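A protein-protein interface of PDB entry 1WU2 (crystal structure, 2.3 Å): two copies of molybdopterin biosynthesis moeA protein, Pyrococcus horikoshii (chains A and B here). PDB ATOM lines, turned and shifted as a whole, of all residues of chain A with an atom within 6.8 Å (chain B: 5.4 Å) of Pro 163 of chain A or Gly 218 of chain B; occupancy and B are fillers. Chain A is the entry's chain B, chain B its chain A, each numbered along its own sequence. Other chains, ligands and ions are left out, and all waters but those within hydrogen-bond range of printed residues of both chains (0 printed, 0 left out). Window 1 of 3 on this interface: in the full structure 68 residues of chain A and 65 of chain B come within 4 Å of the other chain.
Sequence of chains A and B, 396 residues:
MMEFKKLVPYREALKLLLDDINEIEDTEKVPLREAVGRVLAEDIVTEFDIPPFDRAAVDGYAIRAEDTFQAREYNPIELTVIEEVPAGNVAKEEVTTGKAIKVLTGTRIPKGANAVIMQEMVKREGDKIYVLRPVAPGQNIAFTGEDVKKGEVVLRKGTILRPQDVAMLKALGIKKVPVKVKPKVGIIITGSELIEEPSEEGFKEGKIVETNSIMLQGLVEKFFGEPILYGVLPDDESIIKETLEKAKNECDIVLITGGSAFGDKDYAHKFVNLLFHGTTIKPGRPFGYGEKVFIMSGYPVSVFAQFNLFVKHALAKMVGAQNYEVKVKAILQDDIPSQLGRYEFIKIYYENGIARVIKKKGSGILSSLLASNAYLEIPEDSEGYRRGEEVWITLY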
ATOM      1  N   ARG A  33      23.906  19.002  29.597  1.00  0.00           N
ATOM      2  CA  ARG A  33      25.223  18.788  30.206  1.00  0.00           C
ATOM      3  C   ARG A  33      25.281  17.592  31.163  1.00  0.00           C
ATOM      4  O   ARG A  33      26.357  17.052  31.408  1.00  0.00           O
ATOM      5  CB  ARG A  33      25.688  20.057  30.939  1.00  0.00           C
ATOM      6  CG  ARG A  33      27.085  20.516  30.551  1.00  0.00           C
ATOM      7  CD  ARG A  33      28.201  19.560  30.978  1.00  0.00           C
ATOM      8  NE  ARG A  33      29.535  20.108  30.725  1.00  0.00           N
ATOM      9  CZ  ARG A  33      30.120  21.069  31.445  1.00  0.00           C
ATOM     10  NH1 ARG A  33      29.503  21.614  32.493  1.00  0.00           N
ATOM     11  NH2 ARG A  33      31.339  21.487  31.116  1.00  0.00           N
ATOM     12  N   VAL A  36      23.643  12.544  29.678  1.00  0.00           N
ATOM     13  CA  VAL A  36      24.223  11.270  29.247  1.00  0.00           C
ATOM     14  C   VAL A  36      24.038  10.188  30.310  1.00  0.00           C
ATOM     15  O   VAL A  36      24.456  10.358  31.453  1.00  0.00           O
ATOM     16  CB  VAL A  36      25.727  11.410  28.911  1.00  0.00           C
ATOM     17  CG1 VAL A  36      26.379  10.038  28.721  1.00  0.00           C
ATOM     18  CG2 VAL A  36      25.912  12.262  27.667  1.00  0.00           C
ATOM     19  N   LEU A 161      20.812   7.843  26.798  1.00  0.00           N
ATOM     20  CA  LEU A 161      21.435   8.931  26.050  1.00  0.00           C
ATOM     21  C   LEU A 161      22.965   8.832  26.025  1.00  0.00           C
ATOM     22  O   LEU A 161      23.605   8.524  27.025  1.00  0.00           O
ATOM     23  CB  LEU A 161      20.979  10.289  26.597  1.00  0.00           C
ATOM     24  CG  LEU A 161      19.479  10.578  26.444  1.00  0.00           C
ATOM     25  CD1 LEU A 161      19.088  11.834  27.220  1.00  0.00           C
ATOM     26  CD2 LEU A 161      19.093  10.706  24.975  1.00  0.00           C
ATOM     27  N   ARG A 162      23.526   9.077  24.851  1.00  0.00           N
ATOM     28  CA  ARG A 162      24.966   9.051  24.632  1.00  0.00           C
ATOM     29  C   ARG A 162      25.379  10.426  24.120  1.00  0.00           C
ATOM     30  O   ARG A 162      24.523  11.228  23.779  1.00  0.00           O
ATOM     31  CB  ARG A 162      25.307   7.972  23.608  1.00  0.00           C
ATOM     32  CG  ARG A 162      24.849   6.572  23.996  1.00  0.00           C
ATOM     33  CD  ARG A 162      24.818   5.607  22.833  1.00  0.00           C
ATOM     34  NE  ARG A 162      23.965   6.105  21.758  1.00  0.00           N
ATOM     35  CZ  ARG A 162      23.949   5.627  20.518  1.00  0.00           C
ATOM     36  NH1 ARG A 162      24.727   4.613  20.161  1.00  0.00           N
ATOM     37  NH2 ARG A 162      23.138   6.167  19.623  1.00  0.00           N
ATOM     38  N   PRO A 163      26.673  10.718  24.064  1.00  0.00           N
ATOM     39  CA  PRO A 163      27.125  12.014  23.545  1.00  0.00           C
ATOM     40  C   PRO A 163      26.476  12.434  22.213  1.00  0.00           C
ATOM     41  O   PRO A 163      26.115  13.601  22.080  1.00  0.00           O
ATOM     42  CB  PRO A 163      28.629  11.813  23.390  1.00  0.00           C
ATOM     43  CG  PRO A 163      28.972  10.827  24.456  1.00  0.00           C
ATOM     44  CD  PRO A 163      27.806   9.881  24.505  1.00  0.00           C
ATOM     45  N   GLN A 164      26.315  11.504  21.270  1.00  0.00           N
ATOM     46  CA  GLN A 164      25.751  11.825  19.955  1.00  0.00           C
ATOM     47  C   GLN A 164      24.250  12.098  19.995  1.00  0.00           C
ATOM     48  O   GLN A 164      23.757  12.912  19.226  1.00  0.00           O
ATOM     49  CB  GLN A 164      26.076  10.742  18.906  1.00  0.00           C
ATOM     50  CG  GLN A 164      25.526   9.336  19.187  1.00  0.00           C
ATOM     51  CD  GLN A 164      26.600   8.376  19.659  1.00  0.00           C
ATOM     52  OE1 GLN A 164      27.311   8.664  20.618  1.00  0.00           O
ATOM     53  NE2 GLN A 164      26.719   7.231  18.991  1.00  0.00           N
ATOM     54  N   ASP A 165      23.529  11.413  20.878  1.00  0.00           N
ATOM     55  CA  ASP A 165      22.094  11.654  21.056  1.00  0.00           C
ATOM     56  C   ASP A 165      21.849  13.044  21.614  1.00  0.00           C
ATOM     57  O   ASP A 165      20.916  13.733  21.210  1.00  0.00           O
ATOM     58  CB  ASP A 165      21.479  10.646  22.023  1.00  0.00           C
ATOM     59  CG  ASP A 165      21.676   9.217  21.585  1.00  0.00           C
ATOM     60  OD1 ASP A 165      21.438   8.910  20.402  1.00  0.00           O
ATOM     61  OD2 ASP A 165      22.045   8.326  22.368  1.00  0.00           O
ATOM     62  N   VAL A 166      22.688  13.437  22.564  1.00  0.00           N
ATOM     63  CA  VAL A 166      22.604  14.747  23.191  1.00  0.00           C
ATOM     64  C   VAL A 166      22.935  15.821  22.153  1.00  0.00           C
ATOM     65  O   VAL A 166      22.387  16.916  22.198  1.00  0.00           O
ATOM     66  CB  VAL A 166      23.532  14.821  24.424  1.00  0.00           C
ATOM     67  CG1 VAL A 166      23.596  16.229  24.998  1.00  0.00           C
ATOM     68  CG2 VAL A 166      23.045  13.851  25.496  1.00  0.00           C
ATOM     69  N   ALA A 167      23.815  15.482  21.214  1.00  0.00           N
ATOM     70  CA  ALA A 167      24.126  16.338  20.072  1.00  0.00           C
ATOM     71  C   ALA A 167      22.877  16.638  19.249  1.00  0.00           C
ATOM     72  O   ALA A 167      22.639  17.789  18.890  1.00  0.00           O
ATOM     73  CB  ALA A 167      25.176  15.678  19.195  1.00  0.00           C
ATOM     74  N   MET A 168      22.092  15.600  18.958  1.00  0.00           N
ATOM     75  CA  MET A 168      20.838  15.740  18.217  1.00  0.00           C
ATOM     76  C   MET A 168      19.848  16.611  18.971  1.00  0.00           C
ATOM     77  O   MET A 168      19.115  17.375  18.359  1.00  0.00           O
ATOM     78  CB  MET A 168      20.192  14.370  17.953  1.00  0.00           C
ATOM     79  CG  MET A 168      18.864  14.410  17.167  1.00  0.00           C
ATOM     80  SD  MET A 168      18.980  15.173  15.356  1.00  0.00           S
ATOM     81  CE  MET A 168      19.555  13.573  14.379  1.00  0.00           C
ATOM     82  N   SER B 213      30.244  20.887  20.245  1.00  0.00           N
ATOM     83  CA  SER B 213      30.708  21.252  21.575  1.00  0.00           C
ATOM     84  C   SER B 213      30.149  20.287  22.607  1.00  0.00           C
ATOM     85  O   SER B 213      30.903  19.647  23.336  1.00  0.00           O
ATOM     86  CB  SER B 213      30.298  22.679  21.931  1.00  0.00           C
ATOM     87  OG  SER B 213      30.856  23.037  23.181  1.00  0.00           O
ATOM     88  N   ILE B 214      28.825  20.189  22.653  1.00  0.00           N
ATOM     89  CA  ILE B 214      28.147  19.313  23.603  1.00  0.00           C
ATOM     90  C   ILE B 214      28.472  17.833  23.368  1.00  0.00           C
ATOM     91  O   ILE B 214      28.544  17.064  24.324  1.00  0.00           O
ATOM     92  CB  ILE B 214      26.609  19.575  23.604  1.00  0.00           C
ATOM     93  CG1 ILE B 214      25.910  18.794  24.726  1.00  0.00           C
ATOM     94  CG2 ILE B 214      25.976  19.218  22.262  1.00  0.00           C
ATOM     95  CD1 ILE B 214      26.460  19.043  26.111  1.00  0.00           C
ATOM     96  N   MET B 215      28.689  17.442  22.112  1.00  0.00           N
ATOM     97  CA  MET B 215      29.034  16.054  21.802  1.00  0.00           C
ATOM     98  C   MET B 215      30.429  15.717  22.305  1.00  0.00           C
ATOM     99  O   MET B 215      30.647  14.646  22.860  1.00  0.00           O
ATOM    100  CB  MET B 215      28.951  15.763  20.305  1.00  0.00           C
ATOM    101  CG  MET B 215      29.187  14.287  19.983  1.00  0.00           C
ATOM    102  SD  MET B 215      29.052  13.860  18.102  1.00  0.00           S
ATOM    103  CE  MET B 215      30.683  14.709  17.489  1.00  0.00           C
ATOM    104  N   LEU B 216      31.367  16.634  22.103  1.00  0.00           N
ATOM    105  CA  LEU B 216      32.732  16.447  22.578  1.00  0.00           C
ATOM    106  C   LEU B 216      32.828  16.496  24.103  1.00  0.00           C
ATOM    107  O   LEU B 216      33.670  15.824  24.681  1.00  0.00           O
ATOM    108  CB  LEU B 216      33.677  17.479  21.954  1.00  0.00           C
ATOM    109  CG  LEU B 216      34.042  17.233  20.487  1.00  0.00           C
ATOM    110  CD1 LEU B 216      34.762  18.451  19.915  1.00  0.00           C
ATOM    111  CD2 LEU B 216      34.897  15.986  20.334  1.00  0.00           C
ATOM    112  N   GLN B 217      31.968  17.276  24.752  1.00  0.00           N
ATOM    113  CA  GLN B 217      31.938  17.325  26.215  1.00  0.00           C
ATOM    114  C   GLN B 217      31.611  15.940  26.770  1.00  0.00           C
ATOM    115  O   GLN B 217      32.323  15.425  27.621  1.00  0.00           O
ATOM    116  CB  GLN B 217      30.913  18.346  26.717  1.00  0.00           C
ATOM    117  CG  GLN B 217      31.393  19.783  26.632  1.00  0.00           C
ATOM    118  CD  GLN B 217      30.256  20.790  26.678  1.00  0.00           C
ATOM    119  OE1 GLN B 217      29.663  21.017  27.735  1.00  0.00           O
ATOM    120  NE2 GLN B 217      29.954  21.399  25.538  1.00  0.00           N
ATOM    121  N   GLY B 218      30.542  15.338  26.264  1.00  0.00           N
ATOM    122  CA  GLY B 218      30.150  14.000  26.662  1.00  0.00           C
ATOM    123  C   GLY B 218      31.188  12.936  26.354  1.00  0.00           C
ATOM    124  O   GLY B 218      31.393  12.031  27.151  1.00  0.00           O
ATOM    125  N   LEU B 219      31.840  13.053  25.199  1.00  0.00           N
ATOM    126  CA  LEU B 219      32.799  12.049  24.742  1.00  0.00           C
ATOM    127  C   LEU B 219      34.069  12.090  25.584  1.00  0.00           C
ATOM    128  O   LEU B 219      34.654  11.047  25.890  1.00  0.00           O
ATOM    129  CB  LEU B 219      33.143  12.264  23.263  1.00  0.00           C
ATOM    130  CG  LEU B 219      32.106  11.808  22.227  1.00  0.00           C
ATOM    131  CD1 LEU B 219      32.420  12.412  20.859  1.00  0.00           C
ATOM    132  CD2 LEU B 219      32.053  10.293  22.140  1.00  0.00           C
ATOM    133  N   VAL B 220      34.482  13.301  25.960  1.00  0.00           N
ATOM    134  CA  VAL B 220      35.648  13.497  26.813  1.00  0.00           C
ATOM    135  C   VAL B 220      35.361  12.973  28.219  1.00  0.00           C
ATOM    136  O   VAL B 220      36.222  12.355  28.834  1.00  0.00           O
ATOM    137  CB  VAL B 220      36.073  14.986  26.858  1.00  0.00           C
ATOM    138  CG1 VAL B 220      37.075  15.248  27.985  1.00  0.00           C
ATOM    139  CG2 VAL B 220      36.678  15.405  25.526  1.00  0.00           C
ATOM    140  N   GLU B 221      34.150  13.218  28.716  1.00  0.00           N
ATOM    141  CA  GLU B 221      33.733  12.745  30.042  1.00  0.00           C
ATOM    142  C   GLU B 221      33.579  11.223  30.056  1.00  0.00           C
ATOM    143  O   GLU B 221      33.828  10.578  31.074  1.00  0.00           O
ATOM    144  CB  GLU B 221      32.420  13.417  30.483  1.00  0.00           C
ATOM    145  CG  GLU B 221      32.562  14.906  30.787  1.00  0.00           C
ATOM    146  CD  GLU B 221      31.233  15.643  30.928  1.00  0.00           C
ATOM    147  OE1 GLU B 221      30.226  15.225  30.310  1.00  0.00           O
ATOM    148  OE2 GLU B 221      31.193  16.658  31.661  1.00  0.00           O
ATOM    149  N   LYS B 222      33.184  10.653  28.923  1.00  0.00           N
ATOM    150  CA  LYS B 222      33.071   9.203  28.787  1.00  0.00           C
ATOM    151  C   LYS B 222      34.452   8.556  28.866  1.00  0.00           C
ATOM    152  O   LYS B 222      34.597   7.461  29.405  1.00  0.00           O
ATOM    153  CB  LYS B 222      32.391   8.841  27.463  1.00  0.00           C
ATOM    154  CG  LYS B 222      32.201   7.339  27.233  1.00  0.00           C
ATOM    155  CD  LYS B 222      31.647   7.054  25.850  1.00  0.00           C
ATOM    156  CE  LYS B 222      31.469   5.560  25.628  1.00  0.00           C
ATOM    157  NZ  LYS B 222      30.799   5.259  24.334  1.00  0.00           N
ATOM    158  N   PHE B 223      35.459   9.250  28.339  1.00  0.00           N
ATOM    159  CA  PHE B 223      36.816   8.726  28.266  1.00  0.00           C
ATOM    160  C   PHE B 223      37.802   9.528  29.120  1.00  0.00           C
ATOM    161  O   PHE B 223      38.770  10.101  28.606  1.00  0.00           O
ATOM    162  CB  PHE B 223      37.273   8.670  26.805  1.00  0.00           C
ATOM    163  CG  PHE B 223      36.601   7.593  26.009  1.00  0.00           C
ATOM    164  CD1 PHE B 223      36.932   6.260  26.208  1.00  0.00           C
ATOM    165  CD2 PHE B 223      35.624   7.903  25.071  1.00  0.00           C
ATOM    166  CE1 PHE B 223      36.308   5.254  25.477  1.00  0.00           C
ATOM    167  CE2 PHE B 223      34.998   6.901  24.337  1.00  0.00           C
ATOM    168  CZ  PHE B 223      35.343   5.575  24.543  1.00  0.00           C
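OE2 of Glu 221 of chain B is in salt-bridge range of NE of Arg 33 of chain A (3.9 Å).
NE of Arg 33 of chain A lies within hydrogen-bond range of OE1 of Gln 217 of chain B (3.1 Å).
N of Ile 214 of chain B lies close to NE2 of Gln 217 of chain B, 3.3 Å away.
O of Ser 213 of chain B sits at hydrogen-bond distance from NE2 of Gln 217 of chain B (3.0 Å).
Among the printed residues, pairs that only touch across the chains: Val 166 of chain A with Ile 214 of chain B (3.5 Å), Pro 163 of chain A with Met 215 of chain B (3.5 Å), Pro 163 of chain A with Gly 218 of chain B (3.6 Å), Pro 163 of chain A with Leu 219 of chain B (3.7 Å) and Ala 167 of chain A with Met 215 of chain B (3.9 Å).
Of chain B, only Met 215 (3.5 Å), Gly 218 (3.6 Å) and Leu 219 (3.7 Å) come within 4 Å of Pro 163 of chain A.
Of the printed residues of chain B, Val 166 of chain A touches Ile 214 (3.5 Å).
Of the printed residues of chain B, Ala 167 of chain A touches Met 215.
Met 168 of chain A touches none of the printed residues of chain B.
Of the printed residues of chain A, Ile 214 of chain B touches Val 166.
Of the printed residues of chain A, Met 215 of chain B touches Pro 163 (3.5 Å) and Ala 167 (3.9 Å).
Leu 216 of chain B touches none of the printed residues of chain A.
Gly 218 of chain B touches one residue of chain A.
Printed residues of chain A within 4 Å of Glu 221 of chain B: Arg 33.
The nearest residue of chain B that does not touch Pro 163 of chain A is Ile 214 of chain B (4.8 Å).
The nearest residue of chain A that does not touch Gly 218 of chain B is Val 36 of chain A (4.7 Å).
The nearest printed residue of chain A that does not touch Leu 219 of chain B is Gln 164 of chain A (5.2 Å).
Printed residues of chain B that touch a printed residue of chain A: Ile 214, Met 215, Gln 217, Gly 218, Leu 219 and Glu 221.
Hydrophobic or aromatic side chains of chain A within 4 Å of the printed part of chain B: Pro 163, Val 166 and Ala 167.
Among the printed residues, 7 pairs touch across the chains.
No position is printed for both chains.
Of the 7 pairs that touch across the chains among the printed residues, none has its exchanged pair printed and touching as well.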
